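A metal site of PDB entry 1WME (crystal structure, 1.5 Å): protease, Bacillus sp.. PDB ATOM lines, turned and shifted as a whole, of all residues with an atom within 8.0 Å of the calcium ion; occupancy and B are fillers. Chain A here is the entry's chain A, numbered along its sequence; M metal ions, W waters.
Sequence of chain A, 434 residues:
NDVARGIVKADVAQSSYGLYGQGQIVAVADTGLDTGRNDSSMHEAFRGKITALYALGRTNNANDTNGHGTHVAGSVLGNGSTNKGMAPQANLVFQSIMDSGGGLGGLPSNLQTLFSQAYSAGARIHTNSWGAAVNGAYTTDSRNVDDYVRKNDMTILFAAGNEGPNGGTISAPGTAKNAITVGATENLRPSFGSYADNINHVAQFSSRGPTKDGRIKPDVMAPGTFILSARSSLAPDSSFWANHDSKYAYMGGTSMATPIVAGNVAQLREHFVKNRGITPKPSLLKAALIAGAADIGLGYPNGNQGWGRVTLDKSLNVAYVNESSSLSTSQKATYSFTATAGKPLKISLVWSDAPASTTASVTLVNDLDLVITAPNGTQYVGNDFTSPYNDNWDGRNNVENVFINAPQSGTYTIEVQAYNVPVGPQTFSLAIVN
The side-chain carboxylate of Asp 394 sits at hydrogen-bond distance from the backbone NH of Arg 396, at 2.8 Å. The backbone NH (N) of Asp 367 lies within hydrogen-bond range of the backbone carbonyl oxygen (O) of Asn 420, 2.8 Å away. The side-chain carboxylate of Glu 400 sits at hydrogen-bond distance from the backbone NH of Leu 370 (2.8 Å). The side-chain amide nitrogen of Asn 383 is in hydrogen-bond range of the side-chain carboxylate of Asp 394, at 2.9 Å. The backbone carbonyl oxygen of Glu 400 is in hydrogen-bond range of the backbone NH of Leu 349 (2.8 Å). The side-chain carboxylate of Asp 394 sits at hydrogen-bond distance from the backbone NH of Asn 397, at 2.8 Å. N of Asp 369 lies within hydrogen-bond range of O of Gln 417. O of Asp 367 is in hydrogen-bond range of N of Tyr 419.
The nearest printed residue that does not touch the calcium ion is Gly 395 (4.4 Å).
The calcium ion is bound by OE2 of Glu 400 (2.2 Å), OD1 of Asp 367 (2.3 Å), OD1 of Asp 369 (2.3 Å), O of Asp 394 (2.3 Å), O of Leu 368 (2.3 Å) and water W1 (2.4 Å). The calcium ion has six donor atoms within binding distance.
Water W1 lies within hydrogen-bond range of the backbone carbonyl oxygen of Asn 397 (2.7 Å) and the side-chain carboxylate of Asp 394 (2.8 Å).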
ATOM      1  N   LEU A 349     -28.925  28.820  22.431  1.00  0.00           N
ATOM      2  CA  LEU A 349     -28.010  28.569  21.327  1.00  0.00           C
ATOM      3  C   LEU A 349     -28.605  27.446  20.493  1.00  0.00           C
ATOM      4  O   LEU A 349     -28.868  26.342  21.010  1.00  0.00           O
ATOM      5  CB  LEU A 349     -26.637  28.152  21.867  1.00  0.00           C
ATOM      6  CG  LEU A 349     -25.639  27.589  20.841  1.00  0.00           C
ATOM      7  CD1 LEU A 349     -25.219  28.669  19.834  1.00  0.00           C
ATOM      8  CD2 LEU A 349     -24.405  27.013  21.531  1.00  0.00           C
ATOM      9  N   TRP A 351     -28.268  25.462  16.463  1.00  0.00           N
ATOM     10  CA  TRP A 351     -27.596  25.407  15.161  1.00  0.00           C
ATOM     11  C   TRP A 351     -28.299  24.339  14.318  1.00  0.00           C
ATOM     12  O   TRP A 351     -28.873  23.376  14.837  1.00  0.00           O
ATOM     13  CB  TRP A 351     -26.130  25.098  15.306  1.00  0.00           C
ATOM     14  CG  TRP A 351     -25.594  23.857  15.978  1.00  0.00           C
ATOM     15  CD1 TRP A 351     -25.098  22.729  15.374  1.00  0.00           C
ATOM     16  CD2 TRP A 351     -25.477  23.613  17.389  1.00  0.00           C
ATOM     17  NE1 TRP A 351     -24.687  21.820  16.334  1.00  0.00           N
ATOM     18  CE2 TRP A 351     -24.917  22.339  17.587  1.00  0.00           C
ATOM     19  CE3 TRP A 351     -25.819  24.409  18.517  1.00  0.00           C
ATOM     20  CZ2 TRP A 351     -24.680  21.818  18.860  1.00  0.00           C
ATOM     21  CZ3 TRP A 351     -25.576  23.875  19.800  1.00  0.00           C
ATOM     22  CH2 TRP A 351     -25.012  22.597  19.947  1.00  0.00           C
ATOM     23  N   LEU A 364     -25.904  13.804  16.791  1.00  0.00           N
ATOM     24  CA  LEU A 364     -25.201  15.091  16.724  1.00  0.00           C
ATOM     25  C   LEU A 364     -23.897  14.928  15.957  1.00  0.00           C
ATOM     26  O   LEU A 364     -23.133  13.988  16.235  1.00  0.00           O
ATOM     27  CB  LEU A 364     -24.927  15.574  18.142  1.00  0.00           C
ATOM     28  CG  LEU A 364     -24.417  17.016  18.203  1.00  0.00           C
ATOM     29  CD1 LEU A 364     -25.562  17.965  17.797  1.00  0.00           C
ATOM     30  CD2 LEU A 364     -23.836  17.335  19.570  1.00  0.00           C
ATOM     31  N   ASN A 366     -21.886  18.095  14.694  1.00  0.00           N
ATOM     32  CA  ASN A 366     -21.023  19.159  15.198  1.00  0.00           C
ATOM     33  C   ASN A 366     -21.467  19.603  16.586  1.00  0.00           C
ATOM     34  O   ASN A 366     -22.659  19.886  16.774  1.00  0.00           O
ATOM     35  CB  ASN A 366     -21.065  20.348  14.230  1.00  0.00           C
ATOM     36  CG  ASN A 366     -20.517  20.023  12.837  1.00  0.00           C
ATOM     37  OD1 ASN A 366     -19.512  19.303  12.740  1.00  0.00           O
ATOM     38  ND2 ASN A 366     -21.191  20.536  11.804  1.00  0.00           N
ATOM     39  N   ASP A 367     -20.495  19.618  17.484  1.00  0.00           N
ATOM     40  CA  ASP A 367     -20.801  19.897  18.881  1.00  0.00           C
ATOM     41  C   ASP A 367     -20.291  21.277  19.306  1.00  0.00           C
ATOM     42  O   ASP A 367     -19.079  21.485  19.417  1.00  0.00           O
ATOM     43  CB  ASP A 367     -20.175  18.818  19.770  1.00  0.00           C
ATOM     44  CG  ASP A 367     -20.527  18.946  21.226  1.00  0.00           C
ATOM     45  OD1 ASP A 367     -21.309  19.824  21.667  1.00  0.00           O
ATOM     46  OD2 ASP A 367     -19.976  18.152  22.018  1.00  0.00           O
ATOM     47  N   LEU A 368     -21.191  22.198  19.497  1.00  0.00           N
ATOM     48  CA  LEU A 368     -20.917  23.502  20.061  1.00  0.00           C
ATOM     49  C   LEU A 368     -21.360  23.494  21.520  1.00  0.00           C
ATOM     50  O   LEU A 368     -22.292  22.734  21.853  1.00  0.00           O
ATOM     51  CB  LEU A 368     -21.689  24.587  19.328  1.00  0.00           C
ATOM     52  CG  LEU A 368     -21.488  24.681  17.814  1.00  0.00           C
ATOM     53  CD1 LEU A 368     -22.295  25.847  17.244  1.00  0.00           C
ATOM     54  CD2 LEU A 368     -20.017  24.782  17.476  1.00  0.00           C
ATOM     55  N   ASP A 369     -20.684  24.269  22.353  1.00  0.00           N
ATOM     56  CA  ASP A 369     -21.048  24.386  23.740  1.00  0.00           C
ATOM     57  C   ASP A 369     -21.280  25.864  24.085  1.00  0.00           C
ATOM     58  O   ASP A 369     -20.539  26.740  23.640  1.00  0.00           O
ATOM     59  CB  ASP A 369     -19.945  23.828  24.675  1.00  0.00           C
ATOM     60  CG  ASP A 369     -19.758  22.319  24.557  1.00  0.00           C
ATOM     61  OD1 ASP A 369     -20.709  21.580  24.298  1.00  0.00           O
ATOM     62  OD2 ASP A 369     -18.594  21.856  24.729  1.00  0.00           O
ATOM     63  N   LEU A 370     -22.291  26.083  24.918  1.00  0.00           N
ATOM     64  CA  LEU A 370     -22.583  27.434  25.424  1.00  0.00           C
ATOM     65  C   LEU A 370     -22.053  27.624  26.820  1.00  0.00           C
ATOM     66  O   LEU A 370     -22.373  26.810  27.709  1.00  0.00           O
ATOM     67  CB  LEU A 370     -24.121  27.596  25.392  1.00  0.00           C
ATOM     68  CG  LEU A 370     -24.652  28.949  25.894  1.00  0.00           C
ATOM     69  CD1 LEU A 370     -24.225  30.030  24.946  1.00  0.00           C
ATOM     70  CD2 LEU A 370     -26.176  28.860  26.087  1.00  0.00           C
ATOM     71  N   GLY A 382     -24.341  25.165  28.943  1.00  0.00           N
ATOM     72  CA  GLY A 382     -25.592  24.870  28.285  1.00  0.00           C
ATOM     73  C   GLY A 382     -26.288  23.599  28.784  1.00  0.00           C
ATOM     74  O   GLY A 382     -25.615  22.573  28.842  1.00  0.00           O
ATOM     75  N   ASN A 383     -27.576  23.702  29.097  1.00  0.00           N
ATOM     76  CA  ASN A 383     -28.456  22.624  29.552  1.00  0.00           C
ATOM     77  C   ASN A 383     -28.043  22.013  30.888  1.00  0.00           C
ATOM     78  O   ASN A 383     -28.583  20.938  31.245  1.00  0.00           O
ATOM     79  CB  ASN A 383     -28.536  21.532  28.499  1.00  0.00           C
ATOM     80  CG  ASN A 383     -29.210  22.051  27.234  1.00  0.00           C
ATOM     81  OD1 ASN A 383     -29.850  23.111  27.242  1.00  0.00           O
ATOM     82  ND2 ASN A 383     -29.108  21.324  26.131  1.00  0.00           N
ATOM     83  N   TRP A 393     -21.753  18.834  30.898  1.00  0.00           N
ATOM     84  CA  TRP A 393     -21.721  19.413  29.563  1.00  0.00           C
ATOM     85  C   TRP A 393     -22.598  18.659  28.601  1.00  0.00           C
ATOM     86  O   TRP A 393     -22.759  17.436  28.788  1.00  0.00           O
ATOM     87  CB  TRP A 393     -20.285  19.352  29.031  1.00  0.00           C
ATOM     88  CG  TRP A 393     -19.340  20.136  29.894  1.00  0.00           C
ATOM     89  CD1 TRP A 393     -18.819  19.807  31.111  1.00  0.00           C
ATOM     90  CD2 TRP A 393     -18.830  21.419  29.546  1.00  0.00           C
ATOM     91  NE1 TRP A 393     -18.003  20.831  31.530  1.00  0.00           N
ATOM     92  CE2 TRP A 393     -17.994  21.827  30.591  1.00  0.00           C
ATOM     93  CE3 TRP A 393     -19.010  22.243  28.431  1.00  0.00           C
ATOM     94  CZ2 TRP A 393     -17.313  23.050  30.568  1.00  0.00           C
ATOM     95  CZ3 TRP A 393     -18.343  23.461  28.409  1.00  0.00           C
ATOM     96  CH2 TRP A 393     -17.506  23.837  29.474  1.00  0.00           C
ATOM     97  N   ASP A 394     -23.120  19.318  27.598  1.00  0.00           N
ATOM     98  CA  ASP A 394     -24.000  18.623  26.676  1.00  0.00           C
ATOM     99  C   ASP A 394     -23.300  18.219  25.388  1.00  0.00           C
ATOM    100  O   ASP A 394     -22.707  19.087  24.709  1.00  0.00           O
ATOM    101  CB  ASP A 394     -25.170  19.590  26.383  1.00  0.00           C
ATOM    102  CG  ASP A 394     -26.245  18.928  25.552  1.00  0.00           C
ATOM    103  OD1 ASP A 394     -25.933  18.385  24.452  1.00  0.00           O
ATOM    104  OD2 ASP A 394     -27.412  18.970  26.024  1.00  0.00           O
ATOM    105  N   GLY A 395     -23.368  16.932  25.052  1.00  0.00           N
ATOM    106  CA  GLY A 395     -22.778  16.406  23.830  1.00  0.00           C
ATOM    107  C   GLY A 395     -23.808  15.733  22.955  1.00  0.00           C
ATOM    108  O   GLY A 395     -23.472  14.905  22.110  1.00  0.00           O
ATOM    109  N   ARG A 396     -25.090  16.041  23.122  1.00  0.00           N
ATOM    110  CA  ARG A 396     -26.129  15.369  22.368  1.00  0.00           C
ATOM    111  C   ARG A 396     -27.072  16.286  21.617  1.00  0.00           C
ATOM    112  O   ARG A 396     -27.584  15.936  20.525  1.00  0.00           O
ATOM    113  CB  ARG A 396     -27.008  14.509  23.311  1.00  0.00           C
ATOM    114  CG  ARG A 396     -26.273  13.270  23.799  1.00  0.00           C
ATOM    115  CD  ARG A 396     -26.065  12.267  22.641  1.00  0.00           C
ATOM    116  NE  ARG A 396     -25.608  10.968  23.102  1.00  0.00           N
ATOM    117  CZ  ARG A 396     -24.302  10.696  23.133  1.00  0.00           C
ATOM    118  NH1 ARG A 396     -23.462  11.665  22.735  1.00  0.00           N
ATOM    119  NH2 ARG A 396     -23.826   9.537  23.528  1.00  0.00           N
ATOM    120  N   ASN A 397     -27.350  17.473  22.186  1.00  0.00           N
ATOM    121  CA  ASN A 397     -28.382  18.342  21.618  1.00  0.00           C
ATOM    122  C   ASN A 397     -27.812  19.456  20.754  1.00  0.00           C
ATOM    123  O   ASN A 397     -26.747  19.966  21.046  1.00  0.00           O
ATOM    124  CB  ASN A 397     -29.221  18.998  22.744  1.00  0.00           C
ATOM    125  CG  ASN A 397     -30.051  17.964  23.504  1.00  0.00           C
ATOM    126  OD1 ASN A 397     -31.091  17.523  22.946  1.00  0.00           O
ATOM    127  ND2 ASN A 397     -29.586  17.636  24.708  1.00  0.00           N
ATOM    128  N   ASN A 398     -28.530  19.868  19.708  1.00  0.00           N
ATOM    129  CA  ASN A 398     -28.149  21.011  18.905  1.00  0.00           C
ATOM    130  C   ASN A 398     -28.963  22.227  19.341  1.00  0.00           C
ATOM    131  O   ASN A 398     -29.087  23.203  18.568  1.00  0.00           O
ATOM    132  CB  ASN A 398     -28.268  20.761  17.404  1.00  0.00           C
ATOM    133  CG  ASN A 398     -29.655  20.344  16.985  1.00  0.00           C
ATOM    134  OD1 ASN A 398     -30.240  19.459  17.604  1.00  0.00           O
ATOM    135  ND2 ASN A 398     -30.174  20.953  15.902  1.00  0.00           N
ATOM    136  N   VAL A 399     -29.462  22.195  20.566  1.00  0.00           N
ATOM    137  CA  VAL A 399     -30.059  23.309  21.302  1.00  0.00           C
ATOM    138  C   VAL A 399     -29.404  23.337  22.677  1.00  0.00           C
ATOM    139  O   VAL A 399     -29.519  22.282  23.368  1.00  0.00           O
ATOM    140  CB  VAL A 399     -31.588  23.112  21.468  1.00  0.00           C
ATOM    141  CG1 VAL A 399     -32.152  24.283  22.290  1.00  0.00           C
ATOM    142  CG2 VAL A 399     -32.267  22.975  20.098  1.00  0.00           C
ATOM    143  N   GLU A 400     -28.790  24.455  23.087  1.00  0.00           N
ATOM    144  CA  GLU A 400     -28.237  24.557  24.432  1.00  0.00           C
ATOM    145  C   GLU A 400     -28.766  25.831  25.066  1.00  0.00           C
ATOM    146  O   GLU A 400     -28.795  26.850  24.403  1.00  0.00           O
ATOM    147  CB  GLU A 400     -26.714  24.618  24.461  1.00  0.00           C
ATOM    148  CG  GLU A 400     -26.069  23.259  24.238  1.00  0.00           C
ATOM    149  CD  GLU A 400     -24.628  23.124  24.703  1.00  0.00           C
ATOM    150  OE1 GLU A 400     -24.159  24.061  25.394  1.00  0.00           O
ATOM    151  OE2 GLU A 400     -23.997  22.089  24.384  1.00  0.00           O
ATOM    152  N   GLN A 417     -18.467  27.868  22.155  1.00  0.00           N
ATOM    153  CA  GLN A 417     -17.240  27.104  21.964  1.00  0.00           C
ATOM    154  C   GLN A 417     -17.425  25.952  20.993  1.00  0.00           C
ATOM    155  O   GLN A 417     -18.363  25.171  21.146  1.00  0.00           O
ATOM    156  CB  GLN A 417     -16.788  26.554  23.324  1.00  0.00           C
ATOM    157  CG  GLN A 417     -16.678  27.674  24.334  1.00  0.00           C
ATOM    158  CD  GLN A 417     -16.026  27.131  25.601  1.00  0.00           C
ATOM    159  OE1 GLN A 417     -15.921  25.932  25.838  1.00  0.00           O
ATOM    160  NE2 GLN A 417     -15.595  28.073  26.438  1.00  0.00           N
ATOM    161  N   TYR A 419     -16.538  22.617  20.355  1.00  0.00           N
ATOM    162  CA  TYR A 419     -15.841  21.489  20.966  1.00  0.00           C
ATOM    163  C   TYR A 419     -15.297  20.466  19.972  1.00  0.00           C
ATOM    164  O   TYR A 419     -14.179  19.927  20.019  1.00  0.00           O
ATOM    165  CB  TYR A 419     -16.813  20.789  21.936  1.00  0.00           C
ATOM    166  CG  TYR A 419     -16.162  19.596  22.584  1.00  0.00           C
ATOM    167  CD1 TYR A 419     -15.107  19.729  23.490  1.00  0.00           C
ATOM    168  CD2 TYR A 419     -16.626  18.315  22.293  1.00  0.00           C
ATOM    169  CE1 TYR A 419     -14.583  18.570  24.030  1.00  0.00           C
ATOM    170  CE2 TYR A 419     -16.102  17.156  22.833  1.00  0.00           C
ATOM    171  CZ  TYR A 419     -15.060  17.315  23.720  1.00  0.00           C
ATOM    172  OH  TYR A 419     -14.518  16.194  24.278  1.00  0.00           O
ATOM    173  N   ASN A 420     -16.149  20.166  18.967  1.00  0.00           N
ATOM    174  CA  ASN A 420     -15.745  19.201  17.967  1.00  0.00           C
ATOM    175  C   ASN A 420     -16.625  19.406  16.732  1.00  0.00           C
ATOM    176  O   ASN A 420     -17.837  19.179  16.813  1.00  0.00           O
ATOM    177  CB  ASN A 420     -15.899  17.782  18.509  1.00  0.00           C
ATOM    178  CG  ASN A 420     -15.361  16.772  17.505  1.00  0.00           C
ATOM    179  OD1 ASN A 420     -14.462  17.094  16.753  1.00  0.00           O
ATOM    180  ND2 ASN A 420     -15.931  15.578  17.525  1.00  0.00           N
HETATM  181 CA    CA M   1     -22.570  20.849  23.225  1.00  0.00          CA
HETATM  182  O   HOH W   1     -24.464  19.654  22.467  1.00  0.00           O
